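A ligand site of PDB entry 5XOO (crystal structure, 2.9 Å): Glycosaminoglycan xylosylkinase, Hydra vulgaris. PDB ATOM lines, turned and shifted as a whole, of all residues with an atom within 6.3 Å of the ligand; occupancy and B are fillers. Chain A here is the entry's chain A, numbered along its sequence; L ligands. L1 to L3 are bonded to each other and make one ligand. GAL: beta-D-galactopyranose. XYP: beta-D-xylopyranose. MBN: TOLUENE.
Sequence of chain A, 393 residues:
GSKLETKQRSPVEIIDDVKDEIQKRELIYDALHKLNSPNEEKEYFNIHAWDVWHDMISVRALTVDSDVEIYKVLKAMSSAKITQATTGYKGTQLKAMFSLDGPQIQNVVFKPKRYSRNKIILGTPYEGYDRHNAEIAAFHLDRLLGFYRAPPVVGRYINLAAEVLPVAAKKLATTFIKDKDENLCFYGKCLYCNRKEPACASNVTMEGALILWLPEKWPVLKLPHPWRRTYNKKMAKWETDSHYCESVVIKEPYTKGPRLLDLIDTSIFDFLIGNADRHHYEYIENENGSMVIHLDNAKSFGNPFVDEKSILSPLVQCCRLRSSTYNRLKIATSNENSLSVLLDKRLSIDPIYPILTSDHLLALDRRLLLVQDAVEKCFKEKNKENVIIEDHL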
ATOM      1  N   THR A  92      22.507 -12.956  13.672  1.00  0.00           N
ATOM      2  CA  THR A  92      22.951 -11.945  14.613  1.00  0.00           C
ATOM      3  C   THR A  92      24.442 -11.677  14.487  1.00  0.00           C
ATOM      4  O   THR A  92      24.960 -10.820  15.212  1.00  0.00           O
ATOM      5  CB  THR A  92      22.613 -12.372  16.047  1.00  0.00           C
ATOM      6  OG1 THR A  92      23.344 -13.554  16.385  1.00  0.00           O
ATOM      7  CG2 THR A  92      21.125 -12.654  16.183  1.00  0.00           C
ATOM      8  N   GLN A  93      25.132 -12.378  13.600  1.00  0.00           N
ATOM      9  CA  GLN A  93      26.566 -12.279  13.445  1.00  0.00           C
ATOM     10  C   GLN A  93      26.934 -11.795  12.047  1.00  0.00           C
ATOM     11  O   GLN A  93      26.145 -11.868  11.110  1.00  0.00           O
ATOM     12  CB  GLN A  93      27.238 -13.621  13.715  1.00  0.00           C
ATOM     13  CG  GLN A  93      27.060 -14.117  15.130  1.00  0.00           C
ATOM     14  CD  GLN A  93      27.694 -13.199  16.147  1.00  0.00           C
ATOM     15  OE1 GLN A  93      28.665 -12.511  15.855  1.00  0.00           O
ATOM     16  NE2 GLN A  93      27.154 -13.196  17.358  1.00  0.00           N
ATOM     17  N   ARG A 114      38.073 -12.917  13.016  1.00  0.00           N
ATOM     18  CA  ARG A 114      37.803 -11.799  13.899  1.00  0.00           C
ATOM     19  C   ARG A 114      38.700 -11.762  15.132  1.00  0.00           C
ATOM     20  O   ARG A 114      38.730 -10.725  15.817  1.00  0.00           O
ATOM     21  CB  ARG A 114      36.334 -11.808  14.339  1.00  0.00           C
ATOM     22  CG  ARG A 114      35.385 -11.747  13.152  1.00  0.00           C
ATOM     23  CD  ARG A 114      34.087 -11.043  13.460  1.00  0.00           C
ATOM     24  NE  ARG A 114      34.269  -9.614  13.627  1.00  0.00           N
ATOM     25  CZ  ARG A 114      33.275  -8.755  13.794  1.00  0.00           C
ATOM     26  NH1 ARG A 114      32.016  -9.184  13.799  1.00  0.00           N
ATOM     27  NH2 ARG A 114      33.521  -7.459  13.954  1.00  0.00           N
ATOM     28  N   TYR A 115      39.430 -12.827  15.437  1.00  0.00           N
ATOM     29  CA  TYR A 115      40.318 -12.889  16.591  1.00  0.00           C
ATOM     30  C   TYR A 115      41.671 -13.471  16.189  1.00  0.00           C
ATOM     31  O   TYR A 115      41.807 -14.111  15.136  1.00  0.00           O
ATOM     32  CB  TYR A 115      39.751 -13.741  17.735  1.00  0.00           C
ATOM     33  CG  TYR A 115      38.477 -13.240  18.347  1.00  0.00           C
ATOM     34  CD1 TYR A 115      38.480 -12.157  19.208  1.00  0.00           C
ATOM     35  CD2 TYR A 115      37.265 -13.871  18.103  1.00  0.00           C
ATOM     36  CE1 TYR A 115      37.325 -11.696  19.786  1.00  0.00           C
ATOM     37  CE2 TYR A 115      36.096 -13.416  18.687  1.00  0.00           C
ATOM     38  CZ  TYR A 115      36.136 -12.332  19.525  1.00  0.00           C
ATOM     39  OH  TYR A 115      34.985 -11.861  20.106  1.00  0.00           O
ATOM     40  N   THR A 124      30.413 -14.770  29.391  1.00  0.00           N
ATOM     41  CA  THR A 124      29.436 -15.834  29.282  1.00  0.00           C
ATOM     42  C   THR A 124      29.968 -16.973  28.419  1.00  0.00           C
ATOM     43  O   THR A 124      30.859 -16.775  27.590  1.00  0.00           O
ATOM     44  CB  THR A 124      28.135 -15.294  28.706  1.00  0.00           C
ATOM     45  OG1 THR A 124      28.344 -14.889  27.346  1.00  0.00           O
ATOM     46  CG2 THR A 124      27.669 -14.099  29.500  1.00  0.00           C
ATOM     47  N   TYR A 126      28.890 -18.085  25.896  1.00  0.00           N
ATOM     48  CA  TYR A 126      28.559 -17.799  24.499  1.00  0.00           C
ATOM     49  C   TYR A 126      29.124 -16.465  24.059  1.00  0.00           C
ATOM     50  O   TYR A 126      28.646 -15.871  23.093  1.00  0.00           O
ATOM     51  CB  TYR A 126      27.040 -17.832  24.285  1.00  0.00           C
ATOM     52  CG  TYR A 126      26.256 -17.026  25.303  1.00  0.00           C
ATOM     53  CD1 TYR A 126      26.053 -15.660  25.123  1.00  0.00           C
ATOM     54  CD2 TYR A 126      25.727 -17.614  26.435  1.00  0.00           C
ATOM     55  CE1 TYR A 126      25.332 -14.921  26.040  1.00  0.00           C
ATOM     56  CE2 TYR A 126      25.012 -16.881  27.363  1.00  0.00           C
ATOM     57  CZ  TYR A 126      24.816 -15.534  27.160  1.00  0.00           C
ATOM     58  OH  TYR A 126      24.103 -14.799  28.079  1.00  0.00           O
ATOM     59  N   GLU A 127      30.140 -15.964  24.759  1.00  0.00           N
ATOM     60  CA  GLU A 127      30.705 -14.656  24.480  1.00  0.00           C
ATOM     61  C   GLU A 127      31.542 -14.705  23.199  1.00  0.00           C
ATOM     62  O   GLU A 127      32.040 -15.750  22.787  1.00  0.00           O
ATOM     63  CB  GLU A 127      31.587 -14.213  25.650  1.00  0.00           C
ATOM     64  CG  GLU A 127      32.138 -12.788  25.593  1.00  0.00           C
ATOM     65  CD  GLU A 127      31.164 -11.734  26.063  1.00  0.00           C
ATOM     66  OE1 GLU A 127      31.407 -10.539  25.773  1.00  0.00           O
ATOM     67  OE2 GLU A 127      30.165 -12.082  26.733  1.00  0.00           O
ATOM     68  N   GLY A 128      31.684 -13.547  22.583  1.00  0.00           N
ATOM     69  CA  GLY A 128      32.628 -13.355  21.505  1.00  0.00           C
ATOM     70  C   GLY A 128      31.973 -13.333  20.135  1.00  0.00           C
ATOM     71  O   GLY A 128      30.780 -13.638  19.966  1.00  0.00           O
ATOM     72  N   TYR A 129      32.783 -12.989  19.147  1.00  0.00           N
ATOM     73  CA  TYR A 129      32.370 -13.125  17.760  1.00  0.00           C
ATOM     74  C   TYR A 129      32.484 -14.587  17.328  1.00  0.00           C
ATOM     75  O   TYR A 129      33.034 -15.433  18.032  1.00  0.00           O
ATOM     76  CB  TYR A 129      33.241 -12.253  16.856  1.00  0.00           C
ATOM     77  CG  TYR A 129      33.246 -10.771  17.192  1.00  0.00           C
ATOM     78  CD1 TYR A 129      32.064 -10.044  17.207  1.00  0.00           C
ATOM     79  CD2 TYR A 129      34.429 -10.116  17.475  1.00  0.00           C
ATOM     80  CE1 TYR A 129      32.070  -8.699  17.511  1.00  0.00           C
ATOM     81  CE2 TYR A 129      34.436  -8.771  17.779  1.00  0.00           C
ATOM     82  CZ  TYR A 129      33.255  -8.066  17.791  1.00  0.00           C
ATOM     83  OH  TYR A 129      33.271  -6.724  18.097  1.00  0.00           O
ATOM     84  N   ASP A 130      31.958 -14.869  16.143  1.00  0.00           N
ATOM     85  CA  ASP A 130      32.095 -16.197  15.572  1.00  0.00           C
ATOM     86  C   ASP A 130      33.546 -16.445  15.181  1.00  0.00           C
ATOM     87  O   ASP A 130      34.137 -15.670  14.411  1.00  0.00           O
ATOM     88  CB  ASP A 130      31.193 -16.344  14.351  1.00  0.00           C
ATOM     89  CG  ASP A 130      29.745 -16.610  14.725  1.00  0.00           C
ATOM     90  OD1 ASP A 130      29.473 -16.808  15.918  1.00  0.00           O
ATOM     91  OD2 ASP A 130      28.897 -16.632  13.814  1.00  0.00           O
ATOM     92  N   TYR A 192      23.903  -7.383  15.242  1.00  0.00           N
ATOM     93  CA  TYR A 192      24.984  -6.823  16.047  1.00  0.00           C
ATOM     94  C   TYR A 192      26.032  -6.110  15.197  1.00  0.00           C
ATOM     95  O   TYR A 192      27.090  -5.748  15.718  1.00  0.00           O
ATOM     96  CB  TYR A 192      25.636  -7.926  16.877  1.00  0.00           C
ATOM     97  CG  TYR A 192      24.754  -8.485  17.961  1.00  0.00           C
ATOM     98  CD1 TYR A 192      24.009  -7.649  18.785  1.00  0.00           C
ATOM     99  CD2 TYR A 192      24.645  -9.854  18.159  1.00  0.00           C
ATOM    100  CE1 TYR A 192      23.194  -8.157  19.778  1.00  0.00           C
ATOM    101  CE2 TYR A 192      23.835 -10.375  19.150  1.00  0.00           C
ATOM    102  CZ  TYR A 192      23.112  -9.522  19.961  1.00  0.00           C
ATOM    103  OH  TYR A 192      22.304 -10.042  20.943  1.00  0.00           O
ATOM    104  N   GLU A 197      32.517  -2.066  14.651  1.00  0.00           N
ATOM    105  CA  GLU A 197      32.942  -3.446  14.843  1.00  0.00           C
ATOM    106  C   GLU A 197      32.999  -4.161  13.494  1.00  0.00           C
ATOM    107  O   GLU A 197      32.142  -5.007  13.196  1.00  0.00           O
ATOM    108  CB  GLU A 197      32.022  -4.182  15.810  1.00  0.00           C
ATOM    109  CG  GLU A 197      31.680  -3.396  17.060  1.00  0.00           C
ATOM    110  CD  GLU A 197      30.954  -4.246  18.090  1.00  0.00           C
ATOM    111  OE1 GLU A 197      31.256  -5.457  18.190  1.00  0.00           O
ATOM    112  OE2 GLU A 197      30.078  -3.705  18.800  1.00  0.00           O
ATOM    113  N   ARG A 228      18.316 -25.092  26.006  1.00  0.00           N
ATOM    114  CA  ARG A 228      18.819 -23.767  25.666  1.00  0.00           C
ATOM    115  C   ARG A 228      19.105 -22.970  26.933  1.00  0.00           C
ATOM    116  O   ARG A 228      18.524 -23.213  27.995  1.00  0.00           O
ATOM    117  CB  ARG A 228      17.839 -23.022  24.754  1.00  0.00           C
ATOM    118  CG  ARG A 228      16.475 -22.766  25.340  1.00  0.00           C
ATOM    119  CD  ARG A 228      15.546 -22.210  24.265  1.00  0.00           C
ATOM    120  NE  ARG A 228      14.189 -21.992  24.764  1.00  0.00           N
ATOM    121  CZ  ARG A 228      13.268 -22.937  24.850  1.00  0.00           C
ATOM    122  NH1 ARG A 228      13.553 -24.185  24.487  1.00  0.00           N
ATOM    123  NH2 ARG A 228      12.058 -22.645  25.308  1.00  0.00           N
ATOM    124  N   ARG A 229      19.991 -21.989  26.804  1.00  0.00           N
ATOM    125  CA  ARG A 229      20.242 -21.071  27.897  1.00  0.00           C
ATOM    126  C   ARG A 229      19.266 -19.906  27.857  1.00  0.00           C
ATOM    127  O   ARG A 229      18.506 -19.711  26.905  1.00  0.00           O
ATOM    128  CB  ARG A 229      21.680 -20.564  27.869  1.00  0.00           C
ATOM    129  CG  ARG A 229      22.710 -21.655  28.065  1.00  0.00           C
ATOM    130  CD  ARG A 229      24.107 -21.091  28.193  1.00  0.00           C
ATOM    131  NE  ARG A 229      24.985 -22.012  28.901  1.00  0.00           N
ATOM    132  CZ  ARG A 229      25.472 -23.141  28.391  1.00  0.00           C
ATOM    133  NH1 ARG A 229      25.154 -23.516  27.162  1.00  0.00           N
ATOM    134  NH2 ARG A 229      26.262 -23.902  29.127  1.00  0.00           N
ATOM    135  N   TYR A 231      20.072 -16.542  28.300  1.00  0.00           N
ATOM    136  CA  TYR A 231      20.617 -15.336  27.691  1.00  0.00           C
ATOM    137  C   TYR A 231      20.255 -14.080  28.474  1.00  0.00           C
ATOM    138  O   TYR A 231      20.070 -13.004  27.912  1.00  0.00           O
ATOM    139  CB  TYR A 231      20.222 -15.226  26.213  1.00  0.00           C
ATOM    140  CG  TYR A 231      20.894 -16.302  25.408  1.00  0.00           C
ATOM    141  CD1 TYR A 231      22.221 -16.171  25.020  1.00  0.00           C
ATOM    142  CD2 TYR A 231      20.231 -17.488  25.108  1.00  0.00           C
ATOM    143  CE1 TYR A 231      22.850 -17.163  24.302  1.00  0.00           C
ATOM    144  CE2 TYR A 231      20.859 -18.482  24.400  1.00  0.00           C
ATOM    145  CZ  TYR A 231      22.167 -18.320  24.002  1.00  0.00           C
ATOM    146  OH  TYR A 231      22.795 -19.313  23.295  1.00  0.00           O
ATOM    147  N   ASP A 277      26.309 -22.320  22.608  1.00  0.00           N
ATOM    148  CA  ASP A 277      25.396 -21.373  21.990  1.00  0.00           C
ATOM    149  C   ASP A 277      24.366 -22.051  21.084  1.00  0.00           C
ATOM    150  O   ASP A 277      23.799 -21.408  20.200  1.00  0.00           O
ATOM    151  CB  ASP A 277      26.173 -20.325  21.198  1.00  0.00           C
ATOM    152  CG  ASP A 277      25.351 -19.097  20.869  1.00  0.00           C
ATOM    153  OD1 ASP A 277      24.350 -18.849  21.580  1.00  0.00           O
ATOM    154  OD2 ASP A 277      25.701 -18.382  19.917  1.00  0.00           O
ATOM    155  N   HIS A 279      21.193 -22.686  21.055  1.00  0.00           N
ATOM    156  CA  HIS A 279      19.884 -22.430  21.642  1.00  0.00           C
ATOM    157  C   HIS A 279      18.756 -22.920  20.755  1.00  0.00           C
ATOM    158  O   HIS A 279      17.688 -23.279  21.264  1.00  0.00           O
ATOM    159  CB  HIS A 279      19.731 -20.927  21.917  1.00  0.00           C
ATOM    160  CG  HIS A 279      20.097 -20.060  20.765  1.00  0.00           C
ATOM    161  ND1 HIS A 279      19.325 -19.958  19.620  1.00  0.00           N
ATOM    162  CD2 HIS A 279      21.164 -19.245  20.564  1.00  0.00           C
ATOM    163  CE1 HIS A 279      19.906 -19.128  18.774  1.00  0.00           C
ATOM    164  NE2 HIS A 279      21.018 -18.683  19.320  1.00  0.00           N
ATOM    165  N   HIS A 280      18.962 -22.942  19.441  1.00  0.00           N
ATOM    166  CA  HIS A 280      18.038 -23.564  18.493  1.00  0.00           C
ATOM    167  C   HIS A 280      18.812 -24.622  17.723  1.00  0.00           C
ATOM    168  O   HIS A 280      19.815 -24.304  17.080  1.00  0.00           O
ATOM    169  CB  HIS A 280      17.451 -22.532  17.532  1.00  0.00           C
ATOM    170  CG  HIS A 280      16.355 -21.700  18.118  1.00  0.00           C
ATOM    171  ND1 HIS A 280      16.573 -20.823  19.167  1.00  0.00           N
ATOM    172  CD2 HIS A 280      15.040 -21.616  17.819  1.00  0.00           C
ATOM    173  CE1 HIS A 280      15.437 -20.227  19.471  1.00  0.00           C
ATOM    174  NE2 HIS A 280      14.496 -20.689  18.668  1.00  0.00           N
ATOM    175  N   LYS A 299      30.792 -20.562  17.442  1.00  0.00           N
ATOM    176  CA  LYS A 299      30.997 -20.052  18.803  1.00  0.00           C
ATOM    177  C   LYS A 299      31.721 -21.080  19.659  1.00  0.00           C
ATOM    178  O   LYS A 299      31.299 -21.427  20.758  1.00  0.00           O
ATOM    179  CB  LYS A 299      29.671 -19.643  19.421  1.00  0.00           C
ATOM    180  CG  LYS A 299      29.829 -18.669  20.576  1.00  0.00           C
ATOM    181  CD  LYS A 299      29.003 -17.418  20.343  1.00  0.00           C
ATOM    182  CE  LYS A 299      29.487 -16.652  19.137  1.00  0.00           C
ATOM    183  NZ  LYS A 299      28.636 -15.459  18.911  1.00  0.00           N
HETATM  184  C1  GAL L   1      26.751 -12.694  21.020  1.00  0.00           C
HETATM  185  C2  GAL L   1      27.878 -12.783  22.023  1.00  0.00           C
HETATM  186  C3  GAL L   1      28.365 -11.391  22.402  1.00  0.00           C
HETATM  187  C4  GAL L   1      28.627 -10.487  21.171  1.00  0.00           C
HETATM  188  C5  GAL L   1      27.653 -10.761  19.999  1.00  0.00           C
HETATM  189  C6  GAL L   1      28.216 -10.374  18.636  1.00  0.00           C
HETATM  190  O2  GAL L   1      27.480 -13.404  23.217  1.00  0.00           O
HETATM  191  O3  GAL L   1      29.595 -11.469  23.097  1.00  0.00           O
HETATM  192  O4  GAL L   1      29.957 -10.621  20.732  1.00  0.00           O
HETATM  193  O5  GAL L   1      27.278 -12.144  19.861  1.00  0.00           O
HETATM  194  O6  GAL L   1      28.692  -9.031  18.634  1.00  0.00           O
HETATM  195  O1  XYP L   2      21.254 -15.775  20.173  1.00  0.00           O
HETATM  196  C1  XYP L   2      22.534 -15.573  20.582  1.00  0.00           C
HETATM  197  C2  XYP L   2      23.459 -15.673  19.372  1.00  0.00           C
HETATM  198  C3  XYP L   2      24.856 -15.293  19.719  1.00  0.00           C
HETATM  199  C4  XYP L   2      24.911 -13.934  20.345  1.00  0.00           C
HETATM  200  C5  XYP L   2      24.019 -13.852  21.579  1.00  0.00           C
HETATM  201  O2  XYP L   2      23.456 -17.020  18.883  1.00  0.00           O
HETATM  202  O3  XYP L   2      25.653 -15.310  18.507  1.00  0.00           O
HETATM  203  O4  XYP L   2      26.249 -13.966  20.718  1.00  0.00           O
HETATM  204  O5  XYP L   2      22.625 -14.240  21.263  1.00  0.00           O
HETATM  205  C   MBN L   3      20.637 -15.732  21.437  1.00  0.00           C
HETATM  206  C1  MBN L   3      19.229 -16.094  20.988  1.00  0.00           C
HETATM  207  C2  MBN L   3      18.707 -15.537  19.831  1.00  0.00           C
HETATM  208  C3  MBN L   3      17.426 -15.871  19.423  1.00  0.00           C
HETATM  209  C4  MBN L   3      16.676 -16.765  20.172  1.00  0.00           C
HETATM  210  C5  MBN L   3      17.200 -17.321  21.319  1.00  0.00           C
HETATM  211  C6  MBN L   3      18.478 -16.996  21.725  1.00  0.00           C
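NZ of Lys 299 sits close to NE2 of Gln 93.
A ring nitrogen (ND1) of His 280 sits at hydrogen-bond distance from a ring nitrogen (ND1) of His 279 (2.9 Å).
O of Gly 128 sits at hydrogen-bond distance from NZ of Lys 299.
NZ of Lys 299 lies within salt-bridge range of OD1 of Asp 130, 3.4 Å away.
OG1 of Thr 124 lies within hydrogen-bond range of N of Glu 127 (3.3 Å).
The backbone NH (N) of Tyr 129 is in hydrogen-bond range of the side-chain hydroxyl (OH) of Tyr 115 (2.7 Å).
Merely in contact with the ligand: Thr 92 (3.6 Å), Tyr 129 (3.6 Å), Tyr 192 (3.6 Å), Tyr 231 (3.8 Å) and His 280 (3.7 Å).
Of the 19 residues printed, 12 come within 4 Å of the ligand.
The nearest printed residue that does not touch the ligand is Glu 197 (4.4 Å).
NE2 of Gln 93 is in hydrogen-bond range of O5 of GAL L1 (2.7 Å).
The backbone carbonyl oxygen (O) of Tyr 126 is in hydrogen-bond range of an oxygen (O2) of GAL L1, at 2.7 Å.
OD2 of Asp 277 is in hydrogen-bond range of O2 of XYP L2, 2.8 Å away.
O2 of XYP L2 sits at hydrogen-bond distance from NE2 of His 279, 3.0 Å away.
N of Gly 128 lies within hydrogen-bond range of O3 of GAL L1, 3.0 Å away.
O4 of GAL L1 sits at hydrogen-bond distance from O of Gly 128 (3.2 Å).
An oxygen (O3) of XYP L2 sits at hydrogen-bond distance from the side-chain amino group (NZ) of Lys 299, at 3.0 Å.
An oxygen (O3) of GAL L1 is in hydrogen-bond range of the side-chain carboxylate (OE1) of Glu 127 (3.4 Å).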
